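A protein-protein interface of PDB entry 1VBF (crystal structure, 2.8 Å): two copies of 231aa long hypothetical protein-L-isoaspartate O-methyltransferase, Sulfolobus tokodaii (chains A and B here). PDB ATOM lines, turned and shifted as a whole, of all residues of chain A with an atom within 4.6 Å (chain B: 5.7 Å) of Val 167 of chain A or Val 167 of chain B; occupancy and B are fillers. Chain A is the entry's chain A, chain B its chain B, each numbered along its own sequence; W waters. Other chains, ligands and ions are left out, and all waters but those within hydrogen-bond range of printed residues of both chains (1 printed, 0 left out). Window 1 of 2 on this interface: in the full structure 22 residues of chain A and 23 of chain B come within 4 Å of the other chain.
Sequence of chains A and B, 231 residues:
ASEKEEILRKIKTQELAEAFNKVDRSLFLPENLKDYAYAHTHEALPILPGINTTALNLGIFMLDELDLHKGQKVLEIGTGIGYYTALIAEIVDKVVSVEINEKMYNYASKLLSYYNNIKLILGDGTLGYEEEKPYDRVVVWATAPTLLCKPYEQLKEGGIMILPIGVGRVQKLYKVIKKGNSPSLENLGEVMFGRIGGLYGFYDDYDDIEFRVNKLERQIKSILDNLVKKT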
ATOM      1  N   GLY A 166     -27.173 -14.975 -10.500  1.00  0.00           N
ATOM      2  CA  GLY A 166     -25.869 -15.420 -10.076  1.00  0.00           C
ATOM      3  C   GLY A 166     -24.922 -14.307  -9.727  1.00  0.00           C
ATOM      4  O   GLY A 166     -25.010 -13.201 -10.245  1.00  0.00           O
ATOM      5  N   VAL A 167     -24.026 -14.620  -8.803  1.00  0.00           N
ATOM      6  CA  VAL A 167     -23.011 -13.689  -8.353  1.00  0.00           C
ATOM      7  C   VAL A 167     -21.812 -14.231  -9.068  1.00  0.00           C
ATOM      8  O   VAL A 167     -21.787 -15.422  -9.397  1.00  0.00           O
ATOM      9  CB  VAL A 167     -22.774 -13.824  -6.872  1.00  0.00           C
ATOM     10  CG1 VAL A 167     -21.748 -12.816  -6.443  1.00  0.00           C
ATOM     11  CG2 VAL A 167     -24.079 -13.654  -6.127  1.00  0.00           C
ATOM     12  N   GLY A 168     -20.813 -13.416  -9.335  1.00  0.00           N
ATOM     13  CA  GLY A 168     -19.692 -14.002 -10.039  1.00  0.00           C
ATOM     14  C   GLY A 168     -19.672 -13.553 -11.484  1.00  0.00           C
ATOM     15  O   GLY A 168     -20.651 -12.973 -11.956  1.00  0.00           O
ATOM     16  N   ARG A 169     -18.574 -13.831 -12.191  1.00  0.00           N
ATOM     17  CA  ARG A 169     -18.424 -13.381 -13.572  1.00  0.00           C
ATOM     18  C   ARG A 169     -19.146 -14.214 -14.608  1.00  0.00           C
ATOM     19  O   ARG A 169     -19.327 -13.770 -15.734  1.00  0.00           O
ATOM     20  CB  ARG A 169     -16.940 -13.252 -13.929  1.00  0.00           C
ATOM     21  CG  ARG A 169     -16.208 -14.567 -14.104  1.00  0.00           C
ATOM     22  CD  ARG A 169     -14.699 -14.375 -13.986  1.00  0.00           C
ATOM     23  NE  ARG A 169     -13.974 -15.067 -15.041  1.00  0.00           N
ATOM     24  CZ  ARG A 169     -13.938 -14.656 -16.303  1.00  0.00           C
ATOM     25  NH1 ARG A 169     -14.585 -13.557 -16.659  1.00  0.00           N
ATOM     26  NH2 ARG A 169     -13.259 -15.348 -17.208  1.00  0.00           N
ATOM     27  N   ARG A 195     -23.874  -6.683 -13.535  1.00  0.00           N
ATOM     28  CA  ARG A 195     -24.719  -6.792 -12.371  1.00  0.00           C
ATOM     29  C   ARG A 195     -25.838  -5.792 -12.444  1.00  0.00           C
ATOM     30  O   ARG A 195     -25.630  -4.660 -12.881  1.00  0.00           O
ATOM     31  CB  ARG A 195     -23.895  -6.570 -11.116  1.00  0.00           C
ATOM     32  CG  ARG A 195     -23.047  -7.769 -10.784  1.00  0.00           C
ATOM     33  CD  ARG A 195     -22.396  -7.621  -9.428  1.00  0.00           C
ATOM     34  NE  ARG A 195     -21.916  -8.914  -8.952  1.00  0.00           N
ATOM     35  CZ  ARG A 195     -21.376  -9.107  -7.754  1.00  0.00           C
ATOM     36  NH1 ARG A 195     -21.276  -8.069  -6.935  1.00  0.00           N
ATOM     37  NH2 ARG A 195     -20.897 -10.307  -7.399  1.00  0.00           N
ATOM     38  N   PHE A 202     -27.702  -5.731  -6.426  1.00  0.00           N
ATOM     39  CA  PHE A 202     -26.568  -6.156  -5.620  1.00  0.00           C
ATOM     40  C   PHE A 202     -26.155  -5.090  -4.629  1.00  0.00           C
ATOM     41  O   PHE A 202     -26.286  -3.904  -4.899  1.00  0.00           O
ATOM     42  CB  PHE A 202     -25.359  -6.514  -6.497  1.00  0.00           C
ATOM     43  CG  PHE A 202     -25.489  -7.822  -7.218  1.00  0.00           C
ATOM     44  CD1 PHE A 202     -26.228  -7.912  -8.380  1.00  0.00           C
ATOM     45  CD2 PHE A 202     -24.844  -8.951  -6.745  1.00  0.00           C
ATOM     46  CE1 PHE A 202     -26.319  -9.098  -9.066  1.00  0.00           C
ATOM     47  CE2 PHE A 202     -24.926 -10.153  -7.428  1.00  0.00           C
ATOM     48  CZ  PHE A 202     -25.668 -10.228  -8.593  1.00  0.00           C
ATOM     49  N   ASP A 204     -23.091  -5.785  -2.851  1.00  0.00           N
ATOM     50  CA  ASP A 204     -21.633  -5.988  -2.749  1.00  0.00           C
ATOM     51  C   ASP A 204     -21.047  -6.097  -4.165  1.00  0.00           C
ATOM     52  O   ASP A 204     -21.754  -6.454  -5.093  1.00  0.00           O
ATOM     53  CB  ASP A 204     -21.231  -7.236  -1.908  1.00  0.00           C
ATOM     54  CG  ASP A 204     -22.385  -8.206  -1.650  1.00  0.00           C
ATOM     55  OD1 ASP A 204     -23.234  -8.429  -2.539  1.00  0.00           O
ATOM     56  OD2 ASP A 204     -22.426  -8.779  -0.542  1.00  0.00           O
ATOM     57  N   THR B 143     -28.272 -13.893   6.455  1.00  0.00           N
ATOM     58  CA  THR B 143     -28.020 -12.986   5.348  1.00  0.00           C
ATOM     59  C   THR B 143     -28.809 -13.350   4.079  1.00  0.00           C
ATOM     60  O   THR B 143     -29.104 -14.527   3.816  1.00  0.00           O
ATOM     61  CB  THR B 143     -26.474 -12.902   5.060  1.00  0.00           C
ATOM     62  OG1 THR B 143     -26.240 -11.957   4.025  1.00  0.00           O
ATOM     63  CG2 THR B 143     -25.899 -14.248   4.626  1.00  0.00           C
ATOM     64  N   ALA B 144     -29.167 -12.321   3.313  1.00  0.00           N
ATOM     65  CA  ALA B 144     -29.904 -12.491   2.058  1.00  0.00           C
ATOM     66  C   ALA B 144     -29.130 -11.911   0.860  1.00  0.00           C
ATOM     67  O   ALA B 144     -28.251 -11.064   1.023  1.00  0.00           O
ATOM     68  CB  ALA B 144     -31.258 -11.830   2.160  1.00  0.00           C
ATOM     69  N   PRO B 145     -29.446 -12.361  -0.362  1.00  0.00           N
ATOM     70  CA  PRO B 145     -28.720 -11.821  -1.514  1.00  0.00           C
ATOM     71  C   PRO B 145     -29.022 -10.337  -1.705  1.00  0.00           C
ATOM     72  O   PRO B 145     -28.191  -9.585  -2.191  1.00  0.00           O
ATOM     73  CB  PRO B 145     -29.235 -12.670  -2.670  1.00  0.00           C
ATOM     74  CG  PRO B 145     -29.714 -13.957  -1.988  1.00  0.00           C
ATOM     75  CD  PRO B 145     -30.372 -13.435  -0.762  1.00  0.00           C
ATOM     76  N   ILE B 165     -27.411  -8.158   4.682  1.00  0.00           N
ATOM     77  CA  ILE B 165     -27.468  -8.347   3.240  1.00  0.00           C
ATOM     78  C   ILE B 165     -26.076  -8.597   2.670  1.00  0.00           C
ATOM     79  O   ILE B 165     -25.130  -7.861   2.948  1.00  0.00           O
ATOM     80  CB  ILE B 165     -28.053  -7.114   2.503  1.00  0.00           C
ATOM     81  CG1 ILE B 165     -29.490  -6.860   2.953  1.00  0.00           C
ATOM     82  CG2 ILE B 165     -28.002  -7.347   0.980  1.00  0.00           C
ATOM     83  CD1 ILE B 165     -30.086  -5.667   2.285  1.00  0.00           C
ATOM     84  N   GLY B 166     -25.949  -9.640   1.870  1.00  0.00           N
ATOM     85  CA  GLY B 166     -24.664  -9.903   1.275  1.00  0.00           C
ATOM     86  C   GLY B 166     -24.425 -11.315   0.821  1.00  0.00           C
ATOM     87  O   GLY B 166     -24.873 -12.272   1.444  1.00  0.00           O
ATOM     88  N   VAL B 167     -23.759 -11.433  -0.321  1.00  0.00           N
ATOM     89  CA  VAL B 167     -23.354 -12.733  -0.841  1.00  0.00           C
ATOM     90  C   VAL B 167     -21.935 -12.716  -0.253  1.00  0.00           C
ATOM     91  O   VAL B 167     -21.477 -11.666   0.207  1.00  0.00           O
ATOM     92  CB  VAL B 167     -23.351 -12.730  -2.391  1.00  0.00           C
ATOM     93  CG1 VAL B 167     -24.763 -12.696  -2.897  1.00  0.00           C
ATOM     94  CG2 VAL B 167     -22.623 -11.517  -2.923  1.00  0.00           C
ATOM     95  N   GLY B 168     -21.233 -13.827  -0.198  1.00  0.00           N
ATOM     96  CA  GLY B 168     -19.902 -13.732   0.383  1.00  0.00           C
ATOM     97  C   GLY B 168     -19.971 -13.940   1.878  1.00  0.00           C
ATOM     98  O   GLY B 168     -20.954 -13.577   2.512  1.00  0.00           O
ATOM     99  N   ARG B 169     -18.907 -14.509   2.431  1.00  0.00           N
ATOM    100  CA  ARG B 169     -18.820 -14.866   3.834  1.00  0.00           C
ATOM    101  C   ARG B 169     -18.776 -13.752   4.880  1.00  0.00           C
ATOM    102  O   ARG B 169     -18.640 -14.028   6.068  1.00  0.00           O
ATOM    103  CB  ARG B 169     -17.651 -15.834   4.013  1.00  0.00           C
ATOM    104  CG  ARG B 169     -17.057 -16.250   2.673  1.00  0.00           C
ATOM    105  CD  ARG B 169     -17.003 -17.745   2.434  1.00  0.00           C
ATOM    106  NE  ARG B 169     -15.896 -18.377   3.149  1.00  0.00           N
ATOM    107  CZ  ARG B 169     -14.602 -18.084   2.991  1.00  0.00           C
ATOM    108  NH1 ARG B 169     -14.210 -17.153   2.130  1.00  0.00           N
ATOM    109  NH2 ARG B 169     -13.688 -18.725   3.710  1.00  0.00           N
ATOM    110  N   VAL B 170     -18.889 -12.501   4.457  1.00  0.00           N
ATOM    111  CA  VAL B 170     -18.931 -11.381   5.403  1.00  0.00           C
ATOM    112  C   VAL B 170     -19.946 -10.412   4.824  1.00  0.00           C
ATOM    113  O   VAL B 170     -19.763  -9.940   3.720  1.00  0.00           O
ATOM    114  CB  VAL B 170     -17.583 -10.660   5.531  1.00  0.00           C
ATOM    115  CG1 VAL B 170     -17.734  -9.418   6.403  1.00  0.00           C
ATOM    116  CG2 VAL B 170     -16.587 -11.572   6.164  1.00  0.00           C
ATOM    117  N   GLN B 171     -21.007 -10.103   5.557  1.00  0.00           N
ATOM    118  CA  GLN B 171     -22.046  -9.232   5.028  1.00  0.00           C
ATOM    119  C   GLN B 171     -22.160  -7.921   5.764  1.00  0.00           C
ATOM    120  O   GLN B 171     -21.279  -7.553   6.521  1.00  0.00           O
ATOM    121  CB  GLN B 171     -23.391  -9.955   5.078  1.00  0.00           C
ATOM    122  CG  GLN B 171     -23.371 -11.370   4.519  1.00  0.00           C
ATOM    123  CD  GLN B 171     -22.901 -12.393   5.526  1.00  0.00           C
ATOM    124  OE1 GLN B 171     -23.244 -12.325   6.694  1.00  0.00           O
ATOM    125  NE2 GLN B 171     -22.130 -13.362   5.071  1.00  0.00           N
ATOM    126  N   ARG B 195     -26.298 -18.235   5.415  1.00  0.00           N
ATOM    127  CA  ARG B 195     -27.202 -17.874   4.342  1.00  0.00           C
ATOM    128  C   ARG B 195     -28.637 -18.291   4.567  1.00  0.00           C
ATOM    129  O   ARG B 195     -28.905 -19.397   5.038  1.00  0.00           O
ATOM    130  CB  ARG B 195     -26.709 -18.493   3.045  1.00  0.00           C
ATOM    131  CG  ARG B 195     -25.480 -17.837   2.486  1.00  0.00           C
ATOM    132  CD  ARG B 195     -25.129 -18.466   1.180  1.00  0.00           C
ATOM    133  NE  ARG B 195     -24.331 -17.559   0.372  1.00  0.00           N
ATOM    134  CZ  ARG B 195     -24.046 -17.770  -0.907  1.00  0.00           C
ATOM    135  NH1 ARG B 195     -24.494 -18.860  -1.509  1.00  0.00           N
ATOM    136  NH2 ARG B 195     -23.324 -16.883  -1.577  1.00  0.00           N
ATOM    137  N   PHE B 202     -30.329 -17.955  -1.901  1.00  0.00           N
ATOM    138  CA  PHE B 202     -29.251 -17.983  -2.859  1.00  0.00           C
ATOM    139  C   PHE B 202     -29.424 -19.062  -3.900  1.00  0.00           C
ATOM    140  O   PHE B 202     -29.894 -20.154  -3.593  1.00  0.00           O
ATOM    141  CB  PHE B 202     -27.906 -18.131  -2.144  1.00  0.00           C
ATOM    142  CG  PHE B 202     -27.567 -16.969  -1.260  1.00  0.00           C
ATOM    143  CD1 PHE B 202     -28.146 -16.845   0.002  1.00  0.00           C
ATOM    144  CD2 PHE B 202     -26.730 -15.957  -1.710  1.00  0.00           C
ATOM    145  CE1 PHE B 202     -27.906 -15.737   0.791  1.00  0.00           C
ATOM    146  CE2 PHE B 202     -26.476 -14.836  -0.933  1.00  0.00           C
ATOM    147  CZ  PHE B 202     -27.068 -14.724   0.324  1.00  0.00           C
ATOM    148  N   ASP B 204     -26.687 -19.735  -6.118  1.00  0.00           N
ATOM    149  CA  ASP B 204     -25.344 -20.237  -6.415  1.00  0.00           C
ATOM    150  C   ASP B 204     -24.479 -20.208  -5.150  1.00  0.00           C
ATOM    151  O   ASP B 204     -24.836 -19.557  -4.175  1.00  0.00           O
ATOM    152  CB  ASP B 204     -24.697 -19.449  -7.573  1.00  0.00           C
ATOM    153  CG  ASP B 204     -24.715 -17.946  -7.367  1.00  0.00           C
ATOM    154  OD1 ASP B 204     -25.602 -17.448  -6.648  1.00  0.00           O
ATOM    155  OD2 ASP B 204     -23.853 -17.250  -7.951  1.00  0.00           O
ATOM    156  N   TYR B 206     -20.935 -19.744  -2.658  1.00  0.00           N
ATOM    157  CA  TYR B 206     -20.033 -18.657  -2.333  1.00  0.00           C
ATOM    158  C   TYR B 206     -19.014 -18.410  -3.424  1.00  0.00           C
ATOM    159  O   TYR B 206     -18.353 -19.345  -3.883  1.00  0.00           O
ATOM    160  CB  TYR B 206     -19.301 -18.941  -1.029  1.00  0.00           C
ATOM    161  CG  TYR B 206     -20.168 -18.846   0.192  1.00  0.00           C
ATOM    162  CD1 TYR B 206     -20.741 -19.984   0.756  1.00  0.00           C
ATOM    163  CD2 TYR B 206     -20.385 -17.619   0.815  1.00  0.00           C
ATOM    164  CE1 TYR B 206     -21.501 -19.907   1.914  1.00  0.00           C
ATOM    165  CE2 TYR B 206     -21.149 -17.527   1.977  1.00  0.00           C
ATOM    166  CZ  TYR B 206     -21.704 -18.682   2.521  1.00  0.00           C
ATOM    167  OH  TYR B 206     -22.460 -18.600   3.666  1.00  0.00           O
ATOM    168  N   ASP B 207     -18.860 -17.142  -3.801  1.00  0.00           N
ATOM    169  CA  ASP B 207     -17.936 -16.785  -4.864  1.00  0.00           C
ATOM    170  C   ASP B 207     -16.661 -16.046  -4.457  1.00  0.00           C
ATOM    171  O   ASP B 207     -16.386 -14.961  -4.962  1.00  0.00           O
ATOM    172  CB  ASP B 207     -18.673 -15.959  -5.919  1.00  0.00           C
ATOM    173  CG  ASP B 207     -17.858 -15.780  -7.191  1.00  0.00           C
ATOM    174  OD1 ASP B 207     -17.392 -16.808  -7.744  1.00  0.00           O
ATOM    175  OD2 ASP B 207     -17.678 -14.620  -7.638  1.00  0.00           O
HETATM  176  O   HOH W   1     -25.815  -8.010  -2.921  1.00  0.00           O
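OD2 of Asp 204 of chain B sits at hydrogen-bond distance from N of Val 167 of chain A.
The side-chain carboxylate (OD2) of Asp 204 of chain A lies within hydrogen-bond range of the backbone NH (N) of Val 167 of chain B, 3.0 Å away.
Water W1 lies within hydrogen-bond range of OD1 of Asp 204 of chain A (2.6 Å) and O of Pro 145 of chain B (2.9 Å).
Gly 166 of chain A touches Asp 204 of chain B, and with the chains exchanged Asp 204 of chain A touches Gly 166 of chain B.
Val 167 of chain A touches its own counterpart, Val 167 of chain B.
Val 167 of chain A touches Asp 204 of chain B, and with the chains exchanged Asp 204 of chain A touches Val 167 of chain B.
7 positions are printed for both chains.
Of the 6 pairs that touch across the chains among the printed residues, 5 have their exchanged pair printed and touching as well.
Among the printed residues, merely in contact across the chains: Gly 166 of chain A with Asp 204 of chain B, Val 167 of chain A with Val 167 of chain B, Gly 168 of chain A with Asp 207 of chain B and Asp 204 of chain A with Gly 166 of chain B.
Val 167 of chain A touches two residues of chain B.
Of chain A, only Val 167 and Asp 204 come within 4 Å of Val 167 of chain B.
Printed residues of chain A within 4 Å of Asp 207 of chain B: Gly 168 (3.2 Å).
Printed residues of chain A within 4 Å of Asp 204 of chain B: Gly 166 and Val 167.
Of the printed residues of chain B, Gly 168 of chain A touches Asp 207 (3.2 Å).
Thr 143 of chain B touches none of the printed residues of chain A.
The nearest residue of chain B that does not touch Val 167 of chain A is Asp 207 of chain B (4.4 Å).
The nearest printed residue of chain A that does not touch Val 167 of chain B is Arg 195 of chain A (4.9 Å).
The backbone carbonyl oxygen (O) of Asp 204 of chain A sits at hydrogen-bond distance from the guanidinium group (NH1) of Arg 195 of chain A, 2.5 Å away.
OG1 of Thr 143 of chain B lies within hydrogen-bond range of O of Gly 166 of chain B.
The backbone carbonyl oxygen of Ala 144 of chain B is in hydrogen-bond range of the backbone NH of Gly 166 of chain B.
The guanidinium group of Arg 195 of chain B sits at hydrogen-bond distance from the backbone carbonyl oxygen of Asp 204 of chain B (2.8 Å).
Of the 15 printed residues of chain B, 4 touch a printed residue of chain A.
Printed residues of chain B that touch a printed residue of chain A: Gly 166, Val 167, Asp 204 and Asp 207.
Of the 7 printed residues of chain A, 4 touch a printed residue of chain B.
Hydrophobic or aromatic side chains of chain A within 4 Å of the printed part of chain B: Val 167.
Among the printed residues, no Asp or Glu carboxylate lies within 4 Å of a Lys or Arg side-chain nitrogen of the other chain.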
